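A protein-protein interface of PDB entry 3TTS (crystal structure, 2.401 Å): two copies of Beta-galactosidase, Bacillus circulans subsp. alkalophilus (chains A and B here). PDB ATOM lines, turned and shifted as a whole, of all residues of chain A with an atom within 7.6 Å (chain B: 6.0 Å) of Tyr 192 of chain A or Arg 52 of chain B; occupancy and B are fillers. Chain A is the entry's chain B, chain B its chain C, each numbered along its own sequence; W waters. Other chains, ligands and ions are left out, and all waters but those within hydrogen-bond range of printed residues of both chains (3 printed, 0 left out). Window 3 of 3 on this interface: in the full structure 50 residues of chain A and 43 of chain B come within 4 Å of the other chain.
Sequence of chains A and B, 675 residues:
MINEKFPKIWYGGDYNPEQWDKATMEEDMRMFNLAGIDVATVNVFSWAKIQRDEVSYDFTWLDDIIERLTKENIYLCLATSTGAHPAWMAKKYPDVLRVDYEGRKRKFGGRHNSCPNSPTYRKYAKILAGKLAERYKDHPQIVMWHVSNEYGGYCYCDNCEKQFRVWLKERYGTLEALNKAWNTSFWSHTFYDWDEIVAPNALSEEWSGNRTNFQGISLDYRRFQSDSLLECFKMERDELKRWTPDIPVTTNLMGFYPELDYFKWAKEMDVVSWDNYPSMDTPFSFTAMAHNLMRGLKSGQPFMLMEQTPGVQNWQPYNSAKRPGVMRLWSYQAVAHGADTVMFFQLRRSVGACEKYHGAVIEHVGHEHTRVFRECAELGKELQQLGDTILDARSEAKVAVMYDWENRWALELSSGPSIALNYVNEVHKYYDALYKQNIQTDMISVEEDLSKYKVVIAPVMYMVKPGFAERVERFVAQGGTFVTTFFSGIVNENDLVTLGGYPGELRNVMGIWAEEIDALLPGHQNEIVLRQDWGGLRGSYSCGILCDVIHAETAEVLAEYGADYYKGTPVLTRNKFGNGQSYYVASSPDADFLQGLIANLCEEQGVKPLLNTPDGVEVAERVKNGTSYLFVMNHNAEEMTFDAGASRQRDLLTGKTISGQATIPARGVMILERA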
ATOM      1  N   LEU A 175      -9.074 -10.497  22.816  1.00  0.00           N
ATOM      2  CA  LEU A 175      -9.434 -10.124  21.462  1.00  0.00           C
ATOM      3  C   LEU A 175      -9.200 -11.276  20.469  1.00  0.00           C
ATOM      4  O   LEU A 175      -9.944 -11.423  19.499  1.00  0.00           O
ATOM      5  CB  LEU A 175      -8.663  -8.880  21.036  1.00  0.00           C
ATOM      6  CG  LEU A 175      -9.152  -7.598  21.684  1.00  0.00           C
ATOM      7  CD1 LEU A 175      -8.191  -6.494  21.324  1.00  0.00           C
ATOM      8  CD2 LEU A 175     -10.569  -7.267  21.233  1.00  0.00           C
ATOM      9  N   GLU A 176      -8.173 -12.088  20.704  1.00  0.00           N
ATOM     10  CA  GLU A 176      -7.955 -13.268  19.872  1.00  0.00           C
ATOM     11  C   GLU A 176      -9.218 -14.127  19.859  1.00  0.00           C
ATOM     12  O   GLU A 176      -9.715 -14.496  18.802  1.00  0.00           O
ATOM     13  CB  GLU A 176      -6.764 -14.096  20.372  1.00  0.00           C
ATOM     14  CG  GLU A 176      -5.403 -13.385  20.330  1.00  0.00           C
ATOM     15  CD  GLU A 176      -5.314 -12.163  21.266  1.00  0.00           C
ATOM     16  OE1 GLU A 176      -5.681 -12.279  22.464  1.00  0.00           O
ATOM     17  OE2 GLU A 176      -4.877 -11.081  20.795  1.00  0.00           O
ATOM     18  N   LEU A 178     -12.367 -13.321  20.859  1.00  0.00           N
ATOM     19  CA  LEU A 178     -13.489 -12.601  20.270  1.00  0.00           C
ATOM     20  C   LEU A 178     -13.384 -12.542  18.737  1.00  0.00           C
ATOM     21  O   LEU A 178     -14.385 -12.728  18.033  1.00  0.00           O
ATOM     22  CB  LEU A 178     -13.614 -11.187  20.831  1.00  0.00           C
ATOM     23  CG  LEU A 178     -14.686 -10.402  20.058  1.00  0.00           C
ATOM     24  CD1 LEU A 178     -15.693  -9.777  20.985  1.00  0.00           C
ATOM     25  CD2 LEU A 178     -14.067  -9.364  19.122  1.00  0.00           C
ATOM     26  N   ASN A 179     -12.177 -12.280  18.227  1.00  0.00           N
ATOM     27  CA  ASN A 179     -11.981 -12.157  16.782  1.00  0.00           C
ATOM     28  C   ASN A 179     -12.328 -13.458  16.052  1.00  0.00           C
ATOM     29  O   ASN A 179     -13.054 -13.452  15.049  1.00  0.00           O
ATOM     30  CB  ASN A 179     -10.577 -11.654  16.441  1.00  0.00           C
ATOM     31  CG  ASN A 179     -10.482 -10.107  16.414  1.00  0.00           C
ATOM     32  OD1 ASN A 179     -11.400  -9.415  15.966  1.00  0.00           O
ATOM     33  ND2 ASN A 179      -9.363  -9.576  16.890  1.00  0.00           N
ATOM     34  N   HIS A 189     -12.909  -6.972   9.422  1.00  0.00           N
ATOM     35  CA  HIS A 189     -13.490  -6.588  10.709  1.00  0.00           C
ATOM     36  C   HIS A 189     -12.606  -6.863  11.932  1.00  0.00           C
ATOM     37  O   HIS A 189     -13.096  -6.860  13.068  1.00  0.00           O
ATOM     38  CB  HIS A 189     -14.853  -7.260  10.902  1.00  0.00           C
ATOM     39  CG  HIS A 189     -15.995  -6.440  10.390  1.00  0.00           C
ATOM     40  ND1 HIS A 189     -16.024  -5.925   9.110  1.00  0.00           N
ATOM     41  CD2 HIS A 189     -17.132  -6.021  10.993  1.00  0.00           C
ATOM     42  CE1 HIS A 189     -17.142  -5.241   8.943  1.00  0.00           C
ATOM     43  NE2 HIS A 189     -17.830  -5.282  10.069  1.00  0.00           N
ATOM     44  N   THR A 190     -11.315  -7.108  11.699  1.00  0.00           N
ATOM     45  CA  THR A 190     -10.395  -7.394  12.795  1.00  0.00           C
ATOM     46  C   THR A 190     -10.385  -6.258  13.799  1.00  0.00           C
ATOM     47  O   THR A 190     -10.113  -5.111  13.441  1.00  0.00           O
ATOM     48  CB  THR A 190      -8.952  -7.584  12.300  1.00  0.00           C
ATOM     49  OG1 THR A 190      -8.901  -8.648  11.336  1.00  0.00           O
ATOM     50  CG2 THR A 190      -8.040  -7.911  13.462  1.00  0.00           C
ATOM     51  N   PHE A 191     -10.669  -6.578  15.056  1.00  0.00           N
ATOM     52  CA  PHE A 191     -10.601  -5.585  16.123  1.00  0.00           C
ATOM     53  C   PHE A 191      -9.271  -5.707  16.848  1.00  0.00           C
ATOM     54  O   PHE A 191      -8.857  -6.813  17.197  1.00  0.00           O
ATOM     55  CB  PHE A 191     -11.739  -5.800  17.121  1.00  0.00           C
ATOM     56  CG  PHE A 191     -13.115  -5.605  16.539  1.00  0.00           C
ATOM     57  CD1 PHE A 191     -13.600  -4.327  16.287  1.00  0.00           C
ATOM     58  CD2 PHE A 191     -13.932  -6.700  16.275  1.00  0.00           C
ATOM     59  CE1 PHE A 191     -14.872  -4.134  15.763  1.00  0.00           C
ATOM     60  CE2 PHE A 191     -15.215  -6.528  15.752  1.00  0.00           C
ATOM     61  CZ  PHE A 191     -15.688  -5.232  15.501  1.00  0.00           C
ATOM     62  N   TYR A 192      -8.608  -4.575  17.085  1.00  0.00           N
ATOM     63  CA  TYR A 192      -7.344  -4.585  17.820  1.00  0.00           C
ATOM     64  C   TYR A 192      -7.478  -3.971  19.213  1.00  0.00           C
ATOM     65  O   TYR A 192      -6.552  -4.049  20.020  1.00  0.00           O
ATOM     66  CB  TYR A 192      -6.241  -3.859  17.044  1.00  0.00           C
ATOM     67  CG  TYR A 192      -5.781  -4.571  15.795  1.00  0.00           C
ATOM     68  CD1 TYR A 192      -4.958  -5.698  15.869  1.00  0.00           C
ATOM     69  CD2 TYR A 192      -6.151  -4.106  14.540  1.00  0.00           C
ATOM     70  CE1 TYR A 192      -4.538  -6.353  14.718  1.00  0.00           C
ATOM     71  CE2 TYR A 192      -5.732  -4.740  13.388  1.00  0.00           C
ATOM     72  CZ  TYR A 192      -4.922  -5.864  13.479  1.00  0.00           C
ATOM     73  OH  TYR A 192      -4.509  -6.482  12.319  1.00  0.00           O
ATOM     74  N   ASP A 193      -8.624  -3.348  19.471  1.00  0.00           N
ATOM     75  CA  ASP A 193      -8.985  -2.848  20.799  1.00  0.00           C
ATOM     76  C   ASP A 193     -10.494  -3.007  21.006  1.00  0.00           C
ATOM     77  O   ASP A 193     -11.275  -2.890  20.055  1.00  0.00           O
ATOM     78  CB  ASP A 193      -8.592  -1.370  20.970  1.00  0.00           C
ATOM     79  CG  ASP A 193      -8.886  -0.837  22.387  1.00  0.00           C
ATOM     80  OD1 ASP A 193      -8.574  -1.533  23.389  1.00  0.00           O
ATOM     81  OD2 ASP A 193      -9.448   0.278  22.500  1.00  0.00           O
ATOM     82  N   TRP A 194     -10.902  -3.271  22.243  1.00  0.00           N
ATOM     83  CA  TRP A 194     -12.313  -3.430  22.553  1.00  0.00           C
ATOM     84  C   TRP A 194     -13.125  -2.170  22.225  1.00  0.00           C
ATOM     85  O   TRP A 194     -14.312  -2.256  21.887  1.00  0.00           O
ATOM     86  CB  TRP A 194     -12.499  -3.789  24.027  1.00  0.00           C
ATOM     87  CG  TRP A 194     -11.662  -4.938  24.465  1.00  0.00           C
ATOM     88  CD1 TRP A 194     -10.390  -4.888  24.965  1.00  0.00           C
ATOM     89  CD2 TRP A 194     -12.037  -6.317  24.453  1.00  0.00           C
ATOM     90  NE1 TRP A 194      -9.954  -6.153  25.257  1.00  0.00           N
ATOM     91  CE2 TRP A 194     -10.946  -7.048  24.949  1.00  0.00           C
ATOM     92  CE3 TRP A 194     -13.188  -7.002  24.059  1.00  0.00           C
ATOM     93  CZ2 TRP A 194     -10.969  -8.433  25.065  1.00  0.00           C
ATOM     94  CZ3 TRP A 194     -13.216  -8.370  24.180  1.00  0.00           C
ATOM     95  CH2 TRP A 194     -12.110  -9.075  24.677  1.00  0.00           C
ATOM     96  N   ASP A 195     -12.496  -1.003  22.326  1.00  0.00           N
ATOM     97  CA  ASP A 195     -13.230   0.247  22.118  1.00  0.00           C
ATOM     98  C   ASP A 195     -13.638   0.439  20.665  1.00  0.00           C
ATOM     99  O   ASP A 195     -14.418   1.324  20.360  1.00  0.00           O
ATOM    100  CB  ASP A 195     -12.435   1.463  22.612  1.00  0.00           C
ATOM    101  CG  ASP A 195     -12.557   1.672  24.129  1.00  0.00           C
ATOM    102  OD1 ASP A 195     -12.200   2.774  24.602  1.00  0.00           O
ATOM    103  OD2 ASP A 195     -13.017   0.745  24.846  1.00  0.00           O
ATOM    104  N   GLU A 196     -13.101  -0.395  19.775  1.00  0.00           N
ATOM    105  CA  GLU A 196     -13.412  -0.308  18.352  1.00  0.00           C
ATOM    106  C   GLU A 196     -14.734  -0.995  18.047  1.00  0.00           C
ATOM    107  O   GLU A 196     -15.273  -0.854  16.956  1.00  0.00           O
ATOM    108  CB  GLU A 196     -12.302  -0.963  17.524  1.00  0.00           C
ATOM    109  CG  GLU A 196     -10.972  -0.243  17.529  1.00  0.00           C
ATOM    110  CD  GLU A 196      -9.806  -1.132  17.087  1.00  0.00           C
ATOM    111  OE1 GLU A 196     -10.037  -2.207  16.489  1.00  0.00           O
ATOM    112  OE2 GLU A 196      -8.645  -0.756  17.350  1.00  0.00           O
ATOM    113  N   ILE A 197     -15.236  -1.762  19.009  1.00  0.00           N
ATOM    114  CA  ILE A 197     -16.465  -2.524  18.848  1.00  0.00           C
ATOM    115  C   ILE A 197     -17.642  -1.608  19.144  1.00  0.00           C
ATOM    116  O   ILE A 197     -17.593  -0.858  20.110  1.00  0.00           O
ATOM    117  CB  ILE A 197     -16.473  -3.723  19.839  1.00  0.00           C
ATOM    118  CG1 ILE A 197     -15.279  -4.640  19.567  1.00  0.00           C
ATOM    119  CG2 ILE A 197     -17.762  -4.524  19.757  1.00  0.00           C
ATOM    120  CD1 ILE A 197     -15.040  -5.666  20.689  1.00  0.00           C
ATOM    121  N   TRP B  47      -7.677  -5.202   4.773  1.00  0.00           N
ATOM    122  CA  TRP B  47      -7.067  -3.938   5.141  1.00  0.00           C
ATOM    123  C   TRP B  47      -6.608  -3.964   6.612  1.00  0.00           C
ATOM    124  O   TRP B  47      -5.438  -3.662   6.908  1.00  0.00           O
ATOM    125  CB  TRP B  47      -8.029  -2.782   4.848  1.00  0.00           C
ATOM    126  CG  TRP B  47      -7.393  -1.444   4.899  1.00  0.00           C
ATOM    127  CD1 TRP B  47      -6.190  -1.123   5.470  1.00  0.00           C
ATOM    128  CD2 TRP B  47      -7.912  -0.232   4.340  1.00  0.00           C
ATOM    129  NE1 TRP B  47      -5.937   0.217   5.308  1.00  0.00           N
ATOM    130  CE2 TRP B  47      -6.980   0.787   4.616  1.00  0.00           C
ATOM    131  CE3 TRP B  47      -9.081   0.092   3.639  1.00  0.00           C
ATOM    132  CZ2 TRP B  47      -7.179   2.111   4.206  1.00  0.00           C
ATOM    133  CZ3 TRP B  47      -9.278   1.411   3.236  1.00  0.00           C
ATOM    134  CH2 TRP B  47      -8.332   2.399   3.520  1.00  0.00           C
ATOM    135  N   ALA B  48      -7.504  -4.348   7.526  1.00  0.00           N
ATOM    136  CA  ALA B  48      -7.142  -4.428   8.953  1.00  0.00           C
ATOM    137  C   ALA B  48      -6.026  -5.435   9.246  1.00  0.00           C
ATOM    138  O   ALA B  48      -5.187  -5.202  10.111  1.00  0.00           O
ATOM    139  CB  ALA B  48      -8.357  -4.735   9.817  1.00  0.00           C
ATOM    140  N   LYS B  49      -6.025  -6.557   8.533  1.00  0.00           N
ATOM    141  CA  LYS B  49      -4.967  -7.541   8.701  1.00  0.00           C
ATOM    142  C   LYS B  49      -3.640  -6.927   8.319  1.00  0.00           C
ATOM    143  O   LYS B  49      -2.632  -7.143   8.978  1.00  0.00           O
ATOM    144  CB  LYS B  49      -5.221  -8.789   7.854  1.00  0.00           C
ATOM    145  CG  LYS B  49      -4.482 -10.018   8.370  1.00  0.00           C
ATOM    146  CD  LYS B  49      -4.501 -11.169   7.363  1.00  0.00           C
ATOM    147  CE  LYS B  49      -4.060 -12.477   8.022  1.00  0.00           C
ATOM    148  NZ  LYS B  49      -3.192 -12.248   9.216  1.00  0.00           N
ATOM    149  N   ILE B  50      -3.654  -6.141   7.253  1.00  0.00           N
ATOM    150  CA  ILE B  50      -2.446  -5.489   6.789  1.00  0.00           C
ATOM    151  C   ILE B  50      -2.021  -4.346   7.711  1.00  0.00           C
ATOM    152  O   ILE B  50      -0.876  -4.283   8.169  1.00  0.00           O
ATOM    153  CB  ILE B  50      -2.640  -4.938   5.369  1.00  0.00           C
ATOM    154  CG1 ILE B  50      -2.768  -6.095   4.377  1.00  0.00           C
ATOM    155  CG2 ILE B  50      -1.485  -4.031   4.994  1.00  0.00           C
ATOM    156  CD1 ILE B  50      -3.131  -5.665   2.959  1.00  0.00           C
ATOM    157  N   GLN B  51      -2.948  -3.438   7.981  1.00  0.00           N
ATOM    158  CA  GLN B  51      -2.595  -2.187   8.637  1.00  0.00           C
ATOM    159  C   GLN B  51      -3.323  -2.045   9.972  1.00  0.00           C
ATOM    160  O   GLN B  51      -4.511  -1.732   9.998  1.00  0.00           O
ATOM    161  CB  GLN B  51      -2.934  -1.021   7.702  1.00  0.00           C
ATOM    162  CG  GLN B  51      -2.380   0.303   8.155  1.00  0.00           C
ATOM    163  CD  GLN B  51      -2.725   1.454   7.237  1.00  0.00           C
ATOM    164  OE1 GLN B  51      -3.326   1.272   6.172  1.00  0.00           O
ATOM    165  NE2 GLN B  51      -2.343   2.659   7.651  1.00  0.00           N
ATOM    166  N   ARG B  52      -2.621  -2.282  11.076  1.00  0.00           N
ATOM    167  CA  ARG B  52      -3.250  -2.270  12.404  1.00  0.00           C
ATOM    168  C   ARG B  52      -3.304  -0.863  13.057  1.00  0.00           C
ATOM    169  O   ARG B  52      -4.019  -0.633  14.036  1.00  0.00           O
ATOM    170  CB  ARG B  52      -2.559  -3.274  13.332  1.00  0.00           C
ATOM    171  CG  ARG B  52      -1.099  -2.971  13.593  1.00  0.00           C
ATOM    172  CD  ARG B  52      -0.756  -3.144  15.072  1.00  0.00           C
ATOM    173  NE  ARG B  52      -0.810  -4.540  15.508  1.00  0.00           N
ATOM    174  CZ  ARG B  52      -1.244  -4.943  16.705  1.00  0.00           C
ATOM    175  NH1 ARG B  52      -1.689  -4.061  17.604  1.00  0.00           N
ATOM    176  NH2 ARG B  52      -1.241  -6.241  17.000  1.00  0.00           N
ATOM    177  N   ASP B  53      -2.537   0.068  12.516  1.00  0.00           N
ATOM    178  CA  ASP B  53      -2.608   1.458  12.943  1.00  0.00           C
ATOM    179  C   ASP B  53      -2.051   2.318  11.826  1.00  0.00           C
ATOM    180  O   ASP B  53      -1.770   1.814  10.739  1.00  0.00           O
ATOM    181  CB  ASP B  53      -1.856   1.704  14.257  1.00  0.00           C
ATOM    182  CG  ASP B  53      -0.378   1.365  14.173  1.00  0.00           C
ATOM    183  OD1 ASP B  53       0.269   1.649  13.142  1.00  0.00           O
ATOM    184  OD2 ASP B  53       0.143   0.819  15.162  1.00  0.00           O
ATOM    185  N   GLU B  54      -1.886   3.609  12.065  1.00  0.00           N
ATOM    186  CA  GLU B  54      -1.638   4.478  10.934  1.00  0.00           C
ATOM    187  C   GLU B  54      -0.215   4.330  10.428  1.00  0.00           C
ATOM    188  O   GLU B  54       0.151   4.884   9.396  1.00  0.00           O
ATOM    189  CB  GLU B  54      -2.043   5.933  11.208  1.00  0.00           C
ATOM    190  CG  GLU B  54      -1.680   6.478  12.540  1.00  0.00           C
ATOM    191  CD  GLU B  54      -2.674   6.125  13.631  1.00  0.00           C
ATOM    192  OE1 GLU B  54      -3.610   6.918  13.880  1.00  0.00           O
ATOM    193  OE2 GLU B  54      -2.492   5.065  14.262  1.00  0.00           O
ATOM    194  N   SER B  56       1.759   0.987  10.782  1.00  0.00           N
ATOM    195  CA  SER B  56       2.248  -0.393  10.678  1.00  0.00           C
ATOM    196  C   SER B  56       1.651  -1.148   9.495  1.00  0.00           C
ATOM    197  O   SER B  56       0.435  -1.132   9.296  1.00  0.00           O
ATOM    198  CB  SER B  56       1.923  -1.171  11.957  1.00  0.00           C
ATOM    199  OG  SER B  56       2.362  -0.474  13.110  1.00  0.00           O
ATOM    200  N   TYR B  57       2.502  -1.834   8.737  1.00  0.00           N
ATOM    201  CA  TYR B  57       2.048  -2.653   7.612  1.00  0.00           C
ATOM    202  C   TYR B  57       2.707  -4.028   7.628  1.00  0.00           C
ATOM    203  O   TYR B  57       3.930  -4.140   7.578  1.00  0.00           O
ATOM    204  CB  TYR B  57       2.347  -1.971   6.274  1.00  0.00           C
ATOM    205  CG  TYR B  57       1.674  -0.633   6.087  1.00  0.00           C
ATOM    206  CD1 TYR B  57       0.528  -0.514   5.314  1.00  0.00           C
ATOM    207  CD2 TYR B  57       2.189   0.516   6.681  1.00  0.00           C
ATOM    208  CE1 TYR B  57      -0.095   0.703   5.143  1.00  0.00           C
ATOM    209  CE2 TYR B  57       1.578   1.743   6.506  1.00  0.00           C
ATOM    210  CZ  TYR B  57       0.433   1.834   5.736  1.00  0.00           C
ATOM    211  OH  TYR B  57      -0.190   3.063   5.557  1.00  0.00           O
ATOM    212  N   TRP B  88     -10.268   0.347  13.618  1.00  0.00           N
ATOM    213  CA  TRP B  88      -9.486   1.354  14.330  1.00  0.00           C
ATOM    214  C   TRP B  88      -9.565   2.713  13.635  1.00  0.00           C
ATOM    215  O   TRP B  88      -9.619   3.750  14.283  1.00  0.00           O
ATOM    216  CB  TRP B  88      -8.024   0.915  14.541  1.00  0.00           C
ATOM    217  CG  TRP B  88      -7.220   0.737  13.292  1.00  0.00           C
ATOM    218  CD1 TRP B  88      -6.922  -0.435  12.677  1.00  0.00           C
ATOM    219  CD2 TRP B  88      -6.594   1.773  12.506  1.00  0.00           C
ATOM    220  NE1 TRP B  88      -6.150  -0.204  11.557  1.00  0.00           N
ATOM    221  CE2 TRP B  88      -5.931   1.142  11.434  1.00  0.00           C
ATOM    222  CE3 TRP B  88      -6.525   3.170  12.610  1.00  0.00           C
ATOM    223  CZ2 TRP B  88      -5.231   1.855  10.462  1.00  0.00           C
ATOM    224  CZ3 TRP B  88      -5.816   3.879  11.640  1.00  0.00           C
ATOM    225  CH2 TRP B  88      -5.174   3.214  10.586  1.00  0.00           C
ATOM    226  N   LYS B  92     -10.761   6.193  15.223  1.00  0.00           N
ATOM    227  CA  LYS B  92      -9.897   7.361  15.378  1.00  0.00           C
ATOM    228  C   LYS B  92     -10.172   8.453  14.353  1.00  0.00           C
ATOM    229  O   LYS B  92      -9.917   9.626  14.611  1.00  0.00           O
ATOM    230  CB  LYS B  92      -8.424   6.969  15.287  1.00  0.00           C
ATOM    231  CG  LYS B  92      -7.989   5.977  16.317  1.00  0.00           C
ATOM    232  CD  LYS B  92      -6.628   5.425  15.968  1.00  0.00           C
ATOM    233  CE  LYS B  92      -6.224   4.372  16.969  1.00  0.00           C
ATOM    234  NZ  LYS B  92      -4.786   4.084  16.799  1.00  0.00           N
HETATM  235  O   HOH W   1      -9.332  -2.331  14.002  1.00  0.00           O
HETATM  236  O   HOH W   2      -1.248  -6.217  12.045  1.00  0.00           O
HETATM  237  O   HOH W   3      -8.837  -7.964   8.231  1.00  0.00           O
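No position is printed for both chains.
Among the printed residues, merely in contact across the chains: Glu 196 of chain A with Trp 88 of chain B, Tyr 192 of chain A with Arg 52 of chain B, Tyr 192 of chain A with Lys 49 of chain B and Thr 190 of chain A with Ala 48 of chain B.
Printed residues of chain B that touch a printed residue of chain A: Ala 48, Lys 49, Arg 52 and Trp 88.
Hydrophobic or aromatic side chains of chain B that line the printed part of chain A: Ala 48 and Trp 88.
Among the printed residues, 5 pairs touch across the chains.
Among the printed residues, no Asp or Glu carboxylate lies within 4 Å of a Lys or Arg side-chain nitrogen of the other chain.
Of chain B, only Ala 48, Lys 49 and Arg 52 come within 4 Å of Tyr 192 of chain A.
Trp 194 of chain A touches none of the printed residues of chain B.
Of the printed residues of chain B, Glu 196 of chain A touches Trp 88.
Of the printed residues of chain A, Lys 49 of chain B touches Tyr 192.
Of chain A, only Tyr 192 (3.5 Å) comes within 4 Å of Arg 52 of chain B.
Glu 54 of chain B touches none of the printed residues of chain A.
Printed residues of chain A within 4 Å of Trp 88 of chain B: Glu 196.
The nearest residue of chain B that does not touch Tyr 192 of chain A is Trp 88 of chain B (4.2 Å).
The nearest residue of chain A that does not touch Arg 52 of chain B is Glu 196 of chain A (5.7 Å).
OE2 of Glu 196 of chain A sits at hydrogen-bond distance from N of Asp 193 of chain A, at 3.3 Å.
The backbone carbonyl oxygen of Gln 51 of chain B is in hydrogen-bond range of the indole nitrogen of Trp 88 of chain B, 2.7 Å away.
N of Tyr 192 of chain A sits at hydrogen-bond distance from OE1 of Glu 196 of chain A (2.8 Å).
O of Arg 52 of chain B sits close to NE1 of Trp 88 of chain B (3.3 Å).
Water W1 lies within hydrogen-bond range of OE1 of Glu 196 of chain A, N of Trp 88 of chain B and O of Thr 190 of chain A.
Water W3 lies within hydrogen-bond range of the backbone NH of Lys 49 of chain B and the side-chain hydroxyl of Thr 190 of chain A.
Water W2 lies within hydrogen-bond range of the side-chain hydroxyl (OH) of Tyr 192 of chain A (3.3 Å) and the backbone carbonyl oxygen (O) of Lys 49 of chain B (3.5 Å).
The side-chain hydroxyl (OH) of Tyr 192 of chain A sits at hydrogen-bond distance from the backbone carbonyl oxygen (O) of Ala 48 of chain B (2.6 Å).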
